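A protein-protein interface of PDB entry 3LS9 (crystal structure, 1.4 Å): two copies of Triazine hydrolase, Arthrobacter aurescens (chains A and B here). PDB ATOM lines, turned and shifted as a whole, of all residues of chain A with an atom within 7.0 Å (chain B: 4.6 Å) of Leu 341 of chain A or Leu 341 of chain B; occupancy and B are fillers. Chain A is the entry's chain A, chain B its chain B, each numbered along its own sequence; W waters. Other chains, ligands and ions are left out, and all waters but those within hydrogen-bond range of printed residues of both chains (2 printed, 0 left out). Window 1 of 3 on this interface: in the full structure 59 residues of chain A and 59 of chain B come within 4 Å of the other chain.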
ATOM      1  N   ILE A 297     -26.202  23.917   4.811  1.00  0.00           N
ATOM      2  CA  ILE A 297     -25.940  22.782   3.944  1.00  0.00           C
ATOM      3  C   ILE A 297     -27.196  22.260   3.248  1.00  0.00           C
ATOM      4  O   ILE A 297     -27.143  21.892   2.077  1.00  0.00           O
ATOM      5  CB  ILE A 297     -25.242  21.625   4.709  1.00  0.00           C
ATOM      6  CG1 ILE A 297     -24.861  20.485   3.758  1.00  0.00           C
ATOM      7  CG2 ILE A 297     -26.130  21.090   5.847  1.00  0.00           C
ATOM      8  CD1 ILE A 297     -23.722  20.837   2.807  1.00  0.00           C
ATOM      9  N   ALA A 298     -28.328  22.208   3.949  1.00  0.00           N
ATOM     10  CA  ALA A 298     -29.507  21.591   3.343  1.00  0.00           C
ATOM     11  C   ALA A 298     -29.997  22.289   2.071  1.00  0.00           C
ATOM     12  O   ALA A 298     -30.151  21.642   1.046  1.00  0.00           O
ATOM     13  CB  ALA A 298     -30.633  21.418   4.366  1.00  0.00           C
ATOM     14  N   PRO A 299     -30.241  23.608   2.123  1.00  0.00           N
ATOM     15  CA  PRO A 299     -30.657  24.260   0.874  1.00  0.00           C
ATOM     16  C   PRO A 299     -29.545  24.294  -0.175  1.00  0.00           C
ATOM     17  O   PRO A 299     -29.829  24.232  -1.364  1.00  0.00           O
ATOM     18  CB  PRO A 299     -31.026  25.690   1.322  1.00  0.00           C
ATOM     19  CG  PRO A 299     -30.227  25.889   2.564  1.00  0.00           C
ATOM     20  CD  PRO A 299     -30.269  24.548   3.255  1.00  0.00           C
ATOM     21  N   LEU A 301     -27.545  21.984  -0.888  1.00  0.00           N
ATOM     22  CA  LEU A 301     -27.709  20.730  -1.619  1.00  0.00           C
ATOM     23  C   LEU A 301     -29.037  20.686  -2.369  1.00  0.00           C
ATOM     24  O   LEU A 301     -29.086  20.300  -3.543  1.00  0.00           O
ATOM     25  CB  LEU A 301     -27.578  19.523  -0.679  1.00  0.00           C
ATOM     26  CG  LEU A 301     -26.229  19.380   0.032  1.00  0.00           C
ATOM     27  CD1 LEU A 301     -26.212  18.156   0.939  1.00  0.00           C
ATOM     28  CD2 LEU A 301     -25.087  19.344  -0.971  1.00  0.00           C
ATOM     29  N   LEU A 307     -21.164  22.689  -2.410  1.00  0.00           N
ATOM     30  CA  LEU A 307     -20.465  22.728  -1.128  1.00  0.00           C
ATOM     31  C   LEU A 307     -19.728  24.041  -0.901  1.00  0.00           C
ATOM     32  O   LEU A 307     -18.742  24.342  -1.583  1.00  0.00           O
ATOM     33  CB  LEU A 307     -19.462  21.569  -1.033  1.00  0.00           C
ATOM     34  CG  LEU A 307     -20.065  20.170  -1.106  1.00  0.00           C
ATOM     35  CD1 LEU A 307     -18.975  19.127  -1.347  1.00  0.00           C
ATOM     36  CD2 LEU A 307     -20.856  19.876   0.167  1.00  0.00           C
ATOM     37  N   PHE A 322     -24.309  28.193  11.739  1.00  0.00           N
ATOM     38  CA  PHE A 322     -25.093  27.188  11.026  1.00  0.00           C
ATOM     39  C   PHE A 322     -26.561  27.554  11.066  1.00  0.00           C
ATOM     40  O   PHE A 322     -27.039  28.154  12.027  1.00  0.00           O
ATOM     41  CB  PHE A 322     -24.906  25.792  11.647  1.00  0.00           C
ATOM     42  CG  PHE A 322     -24.880  24.678  10.638  1.00  0.00           C
ATOM     43  CD1 PHE A 322     -23.654  24.177  10.222  1.00  0.00           C
ATOM     44  CD2 PHE A 322     -26.042  24.153  10.091  1.00  0.00           C
ATOM     45  CE1 PHE A 322     -23.574  23.161   9.292  1.00  0.00           C
ATOM     46  CE2 PHE A 322     -25.960  23.110   9.144  1.00  0.00           C
ATOM     47  CZ  PHE A 322     -24.721  22.644   8.749  1.00  0.00           C
ATOM     48  N   ASN A 330     -35.903  22.891   2.562  1.00  0.00           N
ATOM     49  CA  ASN A 330     -35.163  22.094   3.527  1.00  0.00           C
ATOM     50  C   ASN A 330     -35.585  20.623   3.608  1.00  0.00           C
ATOM     51  O   ASN A 330     -34.765  19.767   3.301  1.00  0.00           O
ATOM     52  CB  ASN A 330     -35.087  22.768   4.904  1.00  0.00           C
ATOM     53  CG  ASN A 330     -34.235  21.981   5.874  1.00  0.00           C
ATOM     54  OD1 ASN A 330     -34.552  20.840   6.186  1.00  0.00           O
ATOM     55  ND2 ASN A 330     -33.145  22.579   6.343  1.00  0.00           N
ATOM     56  N   ASN A 334     -34.863  21.016  11.353  1.00  0.00           N
ATOM     57  CA  ASN A 334     -34.021  20.153  12.180  1.00  0.00           C
ATOM     58  C   ASN A 334     -32.531  20.465  11.990  1.00  0.00           C
ATOM     59  O   ASN A 334     -31.853  19.884  11.141  1.00  0.00           O
ATOM     60  CB  ASN A 334     -34.332  18.693  11.858  1.00  0.00           C
ATOM     61  CG  ASN A 334     -33.550  17.715  12.714  1.00  0.00           C
ATOM     62  OD1 ASN A 334     -32.806  18.115  13.623  1.00  0.00           O
ATOM     63  ND2 ASN A 334     -33.729  16.428  12.441  1.00  0.00           N
ATOM     64  N   LEU A 336     -29.907  19.944  14.096  1.00  0.00           N
ATOM     65  CA  LEU A 336     -29.024  18.837  14.421  1.00  0.00           C
ATOM     66  C   LEU A 336     -28.936  17.824  13.271  1.00  0.00           C
ATOM     67  O   LEU A 336     -27.854  17.357  12.906  1.00  0.00           O
ATOM     68  CB  LEU A 336     -29.467  18.166  15.725  1.00  0.00           C
ATOM     69  CG  LEU A 336     -28.609  16.968  16.133  1.00  0.00           C
ATOM     70  CD1 LEU A 336     -27.137  17.360  16.223  1.00  0.00           C
ATOM     71  CD2 LEU A 336     -29.107  16.370  17.454  1.00  0.00           C
ATOM     72  N   GLY A 337     -30.077  17.480  12.681  1.00  0.00           N
ATOM     73  CA  GLY A 337     -30.091  16.583  11.540  1.00  0.00           C
ATOM     74  C   GLY A 337     -29.266  17.105  10.378  1.00  0.00           C
ATOM     75  O   GLY A 337     -28.550  16.359   9.708  1.00  0.00           O
ATOM     76  N   ASP A 338     -29.344  18.406  10.138  1.00  0.00           N
ATOM     77  CA  ASP A 338     -28.622  18.981   9.016  1.00  0.00           C
ATOM     78  C   ASP A 338     -27.099  18.924   9.233  1.00  0.00           C
ATOM     79  O   ASP A 338     -26.334  18.878   8.270  1.00  0.00           O
ATOM     80  CB  ASP A 338     -29.093  20.414   8.735  1.00  0.00           C
ATOM     81  CG  ASP A 338     -30.497  20.487   8.113  1.00  0.00           C
ATOM     82  OD1 ASP A 338     -31.145  19.443   7.861  1.00  0.00           O
ATOM     83  OD2 ASP A 338     -30.931  21.630   7.876  1.00  0.00           O
ATOM     84  N   LEU A 339     -26.651  18.926  10.486  1.00  0.00           N
ATOM     85  CA  LEU A 339     -25.214  18.783  10.749  1.00  0.00           C
ATOM     86  C   LEU A 339     -24.683  17.473  10.182  1.00  0.00           C
ATOM     87  O   LEU A 339     -23.555  17.419   9.685  1.00  0.00           O
ATOM     88  CB  LEU A 339     -24.902  18.858  12.249  1.00  0.00           C
ATOM     89  CG  LEU A 339     -25.271  20.176  12.931  1.00  0.00           C
ATOM     90  CD1 LEU A 339     -24.867  20.111  14.402  1.00  0.00           C
ATOM     91  CD2 LEU A 339     -24.624  21.353  12.235  1.00  0.00           C
ATOM     92  N   ARG A 340     -25.470  16.405  10.270  1.00  0.00           N
ATOM     93  CA  ARG A 340     -25.065  15.136   9.670  1.00  0.00           C
ATOM     94  C   ARG A 340     -24.895  15.251   8.160  1.00  0.00           C
ATOM     95  O   ARG A 340     -23.974  14.678   7.593  1.00  0.00           O
ATOM     96  CB  ARG A 340     -26.086  14.047   9.993  1.00  0.00           C
ATOM     97  CG  ARG A 340     -25.790  12.704   9.341  1.00  0.00           C
ATOM     98  CD  ARG A 340     -26.741  11.627   9.844  1.00  0.00           C
ATOM     99  NE  ARG A 340     -26.733  10.419   9.014  1.00  0.00           N
ATOM    100  CZ  ARG A 340     -25.776   9.495   9.016  1.00  0.00           C
ATOM    101  NH1 ARG A 340     -25.887   8.427   8.227  1.00  0.00           N
ATOM    102  NH2 ARG A 340     -24.703   9.635   9.791  1.00  0.00           N
ATOM    103  N   LEU A 341     -25.802  15.968   7.501  1.00  0.00           N
ATOM    104  CA  LEU A 341     -25.678  16.192   6.068  1.00  0.00           C
ATOM    105  C   LEU A 341     -24.337  16.842   5.773  1.00  0.00           C
ATOM    106  O   LEU A 341     -23.650  16.455   4.824  1.00  0.00           O
ATOM    107  CB  LEU A 341     -26.792  17.115   5.563  1.00  0.00           C
ATOM    108  CG  LEU A 341     -28.250  16.690   5.696  1.00  0.00           C
ATOM    109  CD1 LEU A 341     -29.144  17.846   5.274  1.00  0.00           C
ATOM    110  CD2 LEU A 341     -28.535  15.464   4.850  1.00  0.00           C
ATOM    111  N   ALA A 342     -23.958  17.846   6.562  1.00  0.00           N
ATOM    112  CA  ALA A 342     -22.697  18.536   6.314  1.00  0.00           C
ATOM    113  C   ALA A 342     -21.510  17.624   6.612  1.00  0.00           C
ATOM    114  O   ALA A 342     -20.531  17.610   5.867  1.00  0.00           O
ATOM    115  CB  ALA A 342     -22.606  19.824   7.124  1.00  0.00           C
ATOM    116  N   ALA A 343     -21.599  16.841   7.677  1.00  0.00           N
ATOM    117  CA  ALA A 343     -20.490  15.961   8.051  1.00  0.00           C
ATOM    118  C   ALA A 343     -20.160  15.012   6.913  1.00  0.00           C
ATOM    119  O   ALA A 343     -18.990  14.697   6.662  1.00  0.00           O
ATOM    120  CB  ALA A 343     -20.848  15.167   9.295  1.00  0.00           C
ATOM    121  N   LEU A 344     -21.189  14.546   6.225  1.00  0.00           N
ATOM    122  CA  LEU A 344     -20.979  13.557   5.176  1.00  0.00           C
ATOM    123  C   LEU A 344     -20.756  14.195   3.811  1.00  0.00           C
ATOM    124  O   LEU A 344     -19.866  13.786   3.073  1.00  0.00           O
ATOM    125  CB  LEU A 344     -22.141  12.562   5.141  1.00  0.00           C
ATOM    126  CG  LEU A 344     -22.299  11.716   6.406  1.00  0.00           C
ATOM    127  CD1 LEU A 344     -23.553  10.848   6.312  1.00  0.00           C
ATOM    128  CD2 LEU A 344     -21.059  10.851   6.630  1.00  0.00           C
ATOM    129  N   ALA A 345     -21.562  15.192   3.458  1.00  0.00           N
ATOM    130  CA  ALA A 345     -21.551  15.696   2.086  1.00  0.00           C
ATOM    131  C   ALA A 345     -20.265  16.407   1.682  1.00  0.00           C
ATOM    132  O   ALA A 345     -19.930  16.431   0.497  1.00  0.00           O
ATOM    133  CB  ALA A 345     -22.774  16.584   1.814  1.00  0.00           C
ATOM    134  N   HIS A 346     -19.540  16.972   2.641  1.00  0.00           N
ATOM    135  CA  HIS A 346     -18.292  17.657   2.308  1.00  0.00           C
ATOM    136  C   HIS A 346     -17.157  16.698   1.948  1.00  0.00           C
ATOM    137  O   HIS A 346     -16.183  17.108   1.303  1.00  0.00           O
ATOM    138  CB  HIS A 346     -17.822  18.552   3.463  1.00  0.00           C
ATOM    139  CG  HIS A 346     -18.563  19.848   3.563  1.00  0.00           C
ATOM    140  ND1 HIS A 346     -18.235  20.954   2.811  1.00  0.00           N
ATOM    141  CD2 HIS A 346     -19.614  20.212   4.336  1.00  0.00           C
ATOM    142  CE1 HIS A 346     -19.061  21.944   3.110  1.00  0.00           C
ATOM    143  NE2 HIS A 346     -19.905  21.520   4.032  1.00  0.00           N
ATOM    144  N   ARG A 347     -17.264  15.441   2.357  1.00  0.00           N
ATOM    145  CA  ARG A 347     -16.124  14.540   2.249  1.00  0.00           C
ATOM    146  C   ARG A 347     -15.666  14.223   0.822  1.00  0.00           C
ATOM    147  O   ARG A 347     -14.467  14.245   0.553  1.00  0.00           O
ATOM    148  CB  ARG A 347     -16.380  13.281   3.062  1.00  0.00           C
ATOM    149  CG  ARG A 347     -16.647  13.578   4.517  1.00  0.00           C
ATOM    150  CD  ARG A 347     -16.928  12.297   5.282  1.00  0.00           C
ATOM    151  NE  ARG A 347     -17.103  12.556   6.710  1.00  0.00           N
ATOM    152  CZ  ARG A 347     -16.757  11.719   7.681  1.00  0.00           C
ATOM    153  NH1 ARG A 347     -16.215  10.538   7.398  1.00  0.00           N
ATOM    154  NH2 ARG A 347     -16.957  12.065   8.943  1.00  0.00           N
ATOM    155  N   LEU A 363     -18.662  20.932  13.685  1.00  0.00           N
ATOM    156  CA  LEU A 363     -20.044  21.195  13.303  1.00  0.00           C
ATOM    157  C   LEU A 363     -20.890  21.596  14.509  1.00  0.00           C
ATOM    158  O   LEU A 363     -21.683  22.535  14.432  1.00  0.00           O
ATOM    159  CB  LEU A 363     -20.621  19.960  12.619  1.00  0.00           C
ATOM    160  CG  LEU A 363     -20.030  19.746  11.228  1.00  0.00           C
ATOM    161  CD1 LEU A 363     -20.243  18.331  10.783  1.00  0.00           C
ATOM    162  CD2 LEU A 363     -20.632  20.712  10.218  1.00  0.00           C
ATOM    163  N   ILE A 412     -24.040  13.223  15.959  1.00  0.00           N
ATOM    164  CA  ILE A 412     -24.056  13.511  14.529  1.00  0.00           C
ATOM    165  C   ILE A 412     -24.177  12.258  13.662  1.00  0.00           C
ATOM    166  O   ILE A 412     -24.760  12.288  12.573  1.00  0.00           O
ATOM    167  CB  ILE A 412     -22.746  14.227  14.105  1.00  0.00           C
ATOM    168  CG1 ILE A 412     -22.513  15.469  14.962  1.00  0.00           C
ATOM    169  CG2 ILE A 412     -22.771  14.566  12.619  1.00  0.00           C
ATOM    170  CD1 ILE A 412     -23.654  16.444  14.906  1.00  0.00           C
ATOM    171  N   ILE B 297     -25.793   5.305   0.133  1.00  0.00           N
ATOM    172  CA  ILE B 297     -25.325   6.693   0.088  1.00  0.00           C
ATOM    173  C   ILE B 297     -24.461   7.069   1.290  1.00  0.00           C
ATOM    174  O   ILE B 297     -23.477   7.789   1.146  1.00  0.00           O
ATOM    175  CB  ILE B 297     -26.507   7.695  -0.056  1.00  0.00           C
ATOM    176  CG1 ILE B 297     -26.011   9.138  -0.244  1.00  0.00           C
ATOM    177  CG2 ILE B 297     -27.440   7.610   1.149  1.00  0.00           C
ATOM    178  CD1 ILE B 297     -25.327   9.402  -1.584  1.00  0.00           C
ATOM    179  N   ALA B 298     -24.816   6.590   2.478  1.00  0.00           N
ATOM    180  CA  ALA B 298     -24.112   7.056   3.665  1.00  0.00           C
ATOM    181  C   ALA B 298     -22.623   6.680   3.676  1.00  0.00           C
ATOM    182  O   ALA B 298     -21.775   7.550   3.845  1.00  0.00           O
ATOM    183  CB  ALA B 298     -24.811   6.602   4.935  1.00  0.00           C
ATOM    184  N   LEU B 301     -20.589   8.533   0.939  1.00  0.00           N
ATOM    185  CA  LEU B 301     -20.184   9.875   1.353  1.00  0.00           C
ATOM    186  C   LEU B 301     -19.160   9.824   2.490  1.00  0.00           C
ATOM    187  O   LEU B 301     -18.158  10.550   2.480  1.00  0.00           O
ATOM    188  CB  LEU B 301     -21.398  10.705   1.783  1.00  0.00           C
ATOM    189  CG  LEU B 301     -22.467  10.959   0.718  1.00  0.00           C
ATOM    190  CD1 LEU B 301     -23.552  11.857   1.288  1.00  0.00           C
ATOM    191  CD2 LEU B 301     -21.878  11.590  -0.535  1.00  0.00           C
ATOM    192  N   GLY B 337     -33.639   7.761   7.262  1.00  0.00           N
ATOM    193  CA  GLY B 337     -32.815   8.953   7.342  1.00  0.00           C
ATOM    194  C   GLY B 337     -31.826   9.029   6.194  1.00  0.00           C
ATOM    195  O   GLY B 337     -31.562  10.107   5.644  1.00  0.00           O
ATOM    196  N   ASP B 338     -31.262   7.889   5.816  1.00  0.00           N
ATOM    197  CA  ASP B 338     -30.285   7.894   4.730  1.00  0.00           C
ATOM    198  C   ASP B 338     -30.908   8.265   3.375  1.00  0.00           C
ATOM    199  O   ASP B 338     -30.224   8.798   2.499  1.00  0.00           O
ATOM    200  CB  ASP B 338     -29.544   6.560   4.642  1.00  0.00           C
ATOM    201  CG  ASP B 338     -28.549   6.355   5.783  1.00  0.00           C
ATOM    202  OD1 ASP B 338     -28.378   7.248   6.653  1.00  0.00           O
ATOM    203  OD2 ASP B 338     -27.929   5.268   5.791  1.00  0.00           O
ATOM    204  N   LEU B 339     -32.201   7.998   3.196  1.00  0.00           N
ATOM    205  CA  LEU B 339     -32.879   8.405   1.972  1.00  0.00           C
ATOM    206  C   LEU B 339     -32.806   9.910   1.784  1.00  0.00           C
ATOM    207  O   LEU B 339     -32.656  10.386   0.661  1.00  0.00           O
ATOM    208  CB  LEU B 339     -34.340   7.966   1.978  1.00  0.00           C
ATOM    209  CG  LEU B 339     -34.553   6.453   1.960  1.00  0.00           C
ATOM    210  CD1 LEU B 339     -36.041   6.168   1.860  1.00  0.00           C
ATOM    211  CD2 LEU B 339     -33.810   5.774   0.816  1.00  0.00           C
ATOM    212  N   ARG B 340     -32.922  10.667   2.874  1.00  0.00           N
ATOM    213  CA  ARG B 340     -32.834  12.118   2.785  1.00  0.00           C
ATOM    214  C   ARG B 340     -31.444  12.537   2.321  1.00  0.00           C
ATOM    215  O   ARG B 340     -31.290  13.452   1.504  1.00  0.00           O
ATOM    216  CB  ARG B 340     -33.144  12.743   4.140  1.00  0.00           C
ATOM    217  CG  ARG B 340     -32.926  14.238   4.188  1.00  0.00           C
ATOM    218  CD  ARG B 340     -33.422  14.802   5.509  1.00  0.00           C
ATOM    219  NE  ARG B 340     -32.948  16.163   5.746  1.00  0.00           N
ATOM    220  CZ  ARG B 340     -33.425  17.253   5.147  1.00  0.00           C
ATOM    221  NH1 ARG B 340     -32.918  18.445   5.450  1.00  0.00           N
ATOM    222  NH2 ARG B 340     -34.392  17.148   4.233  1.00  0.00           N
ATOM    223  N   LEU B 341     -30.425  11.864   2.837  1.00  0.00           N
ATOM    224  CA  LEU B 341     -29.073  12.123   2.384  1.00  0.00           C
ATOM    225  C   LEU B 341     -28.972  11.958   0.865  1.00  0.00           C
ATOM    226  O   LEU B 341     -28.375  12.796   0.187  1.00  0.00           O
ATOM    227  CB  LEU B 341     -28.102  11.175   3.089  1.00  0.00           C
ATOM    228  CG  LEU B 341     -26.618  11.484   2.949  1.00  0.00           C
ATOM    229  CD1 LEU B 341     -26.304  12.888   3.452  1.00  0.00           C
ATOM    230  CD2 LEU B 341     -25.824  10.447   3.722  1.00  0.00           C
ATOM    231  N   ALA B 342     -29.551  10.889   0.325  1.00  0.00           N
ATOM    232  CA  ALA B 342     -29.497  10.657  -1.113  1.00  0.00           C
ATOM    233  C   ALA B 342     -30.313  11.685  -1.884  1.00  0.00           C
ATOM    234  O   ALA B 342     -29.886  12.156  -2.951  1.00  0.00           O
ATOM    235  CB  ALA B 342     -29.956   9.241  -1.459  1.00  0.00           C
ATOM    236  N   ALA B 343     -31.481  12.035  -1.354  1.00  0.00           N
ATOM    237  CA  ALA B 343     -32.331  13.014  -2.022  1.00  0.00           C
ATOM    238  C   ALA B 343     -31.586  14.313  -2.253  1.00  0.00           C
ATOM    239  O   ALA B 343     -31.750  14.959  -3.286  1.00  0.00           O
ATOM    240  CB  ALA B 343     -33.576  13.285  -1.193  1.00  0.00           C
ATOM    241  N   LEU B 344     -30.778  14.712  -1.280  1.00  0.00           N
ATOM    242  CA  LEU B 344     -30.111  16.002  -1.360  1.00  0.00           C
ATOM    243  C   LEU B 344     -28.743  15.919  -2.025  1.00  0.00           C
ATOM    244  O   LEU B 344     -28.396  16.747  -2.868  1.00  0.00           O
ATOM    245  CB  LEU B 344     -30.008  16.638   0.032  1.00  0.00           C
ATOM    246  CG  LEU B 344     -31.346  16.974   0.704  1.00  0.00           C
ATOM    247  CD1 LEU B 344     -31.123  17.507   2.120  1.00  0.00           C
ATOM    248  CD2 LEU B 344     -32.167  17.950  -0.128  1.00  0.00           C
ATOM    249  N   ALA B 345     -27.954  14.922  -1.646  1.00  0.00           N
ATOM    250  CA  ALA B 345     -26.558  14.898  -2.056  1.00  0.00           C
ATOM    251  C   ALA B 345     -26.348  14.679  -3.550  1.00  0.00           C
ATOM    252  O   ALA B 345     -25.333  15.117  -4.096  1.00  0.00           O
ATOM    253  CB  ALA B 345     -25.784  13.866  -1.243  1.00  0.00           C
HETATM  254  O   HOH W   1     -31.280  16.642   7.892  1.00  0.00           O
HETATM  255  O   HOH W   2     -29.036   9.718   7.707  1.00  0.00           O
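The backbone carbonyl oxygen (O) of Asn 330 of chain A lies within hydrogen-bond range of the guanidinium group (NH2) of Arg 340 of chain B.
OD1 of Asp 338 of chain A lies within salt-bridge range of NH1 of Arg 340 of chain B (3.2 Å).
NH1 of Arg 340 of chain A is in salt-bridge range of OD1 of Asp 338 of chain B (3.2 Å).
Printed residues of chain A that touch a printed residue of chain B: Ala 298, Leu 301, Asn 330, Asp 338, Arg 340, Leu 341, Leu 344 and Arg 347.
Hydrophobic or aromatic side chains of chain A within 4 Å of the printed part of chain B: Ala 298, Leu 301, Leu 341 and Leu 344.
Of the 12 printed residues of chain B, 6 touch a printed residue of chain A.
Among the printed residues, Asp or Glu carboxylates within 4 Å of a Lys or Arg side-chain nitrogen of the other chain: Asp 338 of chain A with Arg 340 of chain B (3.2 Å) and Arg 340 of chain A with Asp 338 of chain B (3.2 Å).
Water W2 lies within hydrogen-bond range of the guanidinium group (NE) of Arg 340 of chain A (2.7 Å), the side-chain carboxylate (OD1) of Asp 338 of chain B (2.8 Å) and the backbone carbonyl oxygen (O) of Gly 337 of chain B (3.3 Å).
Water W1 lies within hydrogen-bond range of the guanidinium group (NE) of Arg 340 of chain B (2.8 Å), the side-chain carboxylate (OD1) of Asp 338 of chain A (2.8 Å) and the backbone carbonyl oxygen (O) of Gly 337 of chain A (3.3 Å).
Ala 298 of chain A touches Arg 340 of chain B, and with the chains exchanged Arg 340 of chain A touches Ala 298 of chain B.
Leu 341 of chain A touches Arg 340 of chain B, but with the chains exchanged Arg 340 of chain A does not touch Leu 341 of chain B (4.9 Å).
Leu 341 of chain A touches its own counterpart, Leu 341 of chain B.
Leu 341 of chain A touches Leu 344 of chain B, and with the chains exchanged Leu 344 of chain A touches Leu 341 of chain B.
Positions printed for both chains: 297, 298, 301, 337, 338, 339, 340, 341, 342, 343, 344 and 345.
Printed residues of chain B within 4 Å of Ala 298 of chain A: Arg 340 (3.9 Å).
Of the printed residues of chain B, Asp 338 of chain A touches Arg 340 (3.2 Å).
Printed residues of chain B within 4 Å of Arg 340 of chain A: Ala 298 (3.9 Å) and Asp 338 (3.2 Å).
Printed residues of chain B within 4 Å of Leu 341 of chain A: Arg 340 (3.8 Å), Leu 341 (3.7 Å) and Leu 344 (3.7 Å).
Of the printed residues of chain A, Ala 298 of chain B touches Arg 340.
Of chain A, only Leu 341 (3.7 Å) and Leu 344 (3.5 Å) come within 4 Å of Leu 341 of chain B.
Of the printed residues of chain A, Leu 344 of chain B touches Leu 301 and Leu 341.
The nearest residue of chain A that does not touch Leu 341 of chain B is Arg 340 of chain A (4.9 Å).
The nearest printed residue of chain B that does not touch Asn 330 of chain A is Leu 344 of chain B (4.4 Å).
OD2 of Asp 338 of chain A lies within hydrogen-bond range of ND2 of Asn 330 of chain A, 2.9 Å away.
The guanidinium group (NE) of Arg 347 of chain A sits at hydrogen-bond distance from the backbone carbonyl oxygen (O) of Ala 343 of chain A.
Among the printed residues, pairs that only touch across the chains: Ala 298 of chain A with Arg 340 of chain B (3.9 Å), Leu 301 of chain A with Leu 344 of chain B (3.6 Å), Arg 340 of chain A with Ala 298 of chain B (3.9 Å), Leu 341 of chain A with Arg 340 of chain B (3.8 Å), Leu 341 of chain A with Leu 341 of chain B (3.7 Å), Leu 341 of chain A with Leu 344 of chain B (3.7 Å), Leu 344 of chain A with Leu 301 of chain B (3.7 Å), Leu 344 of chain A with Leu 341 of chain B (3.5 Å) and Arg 347 of chain A with Leu 301 of chain B (3.3 Å).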
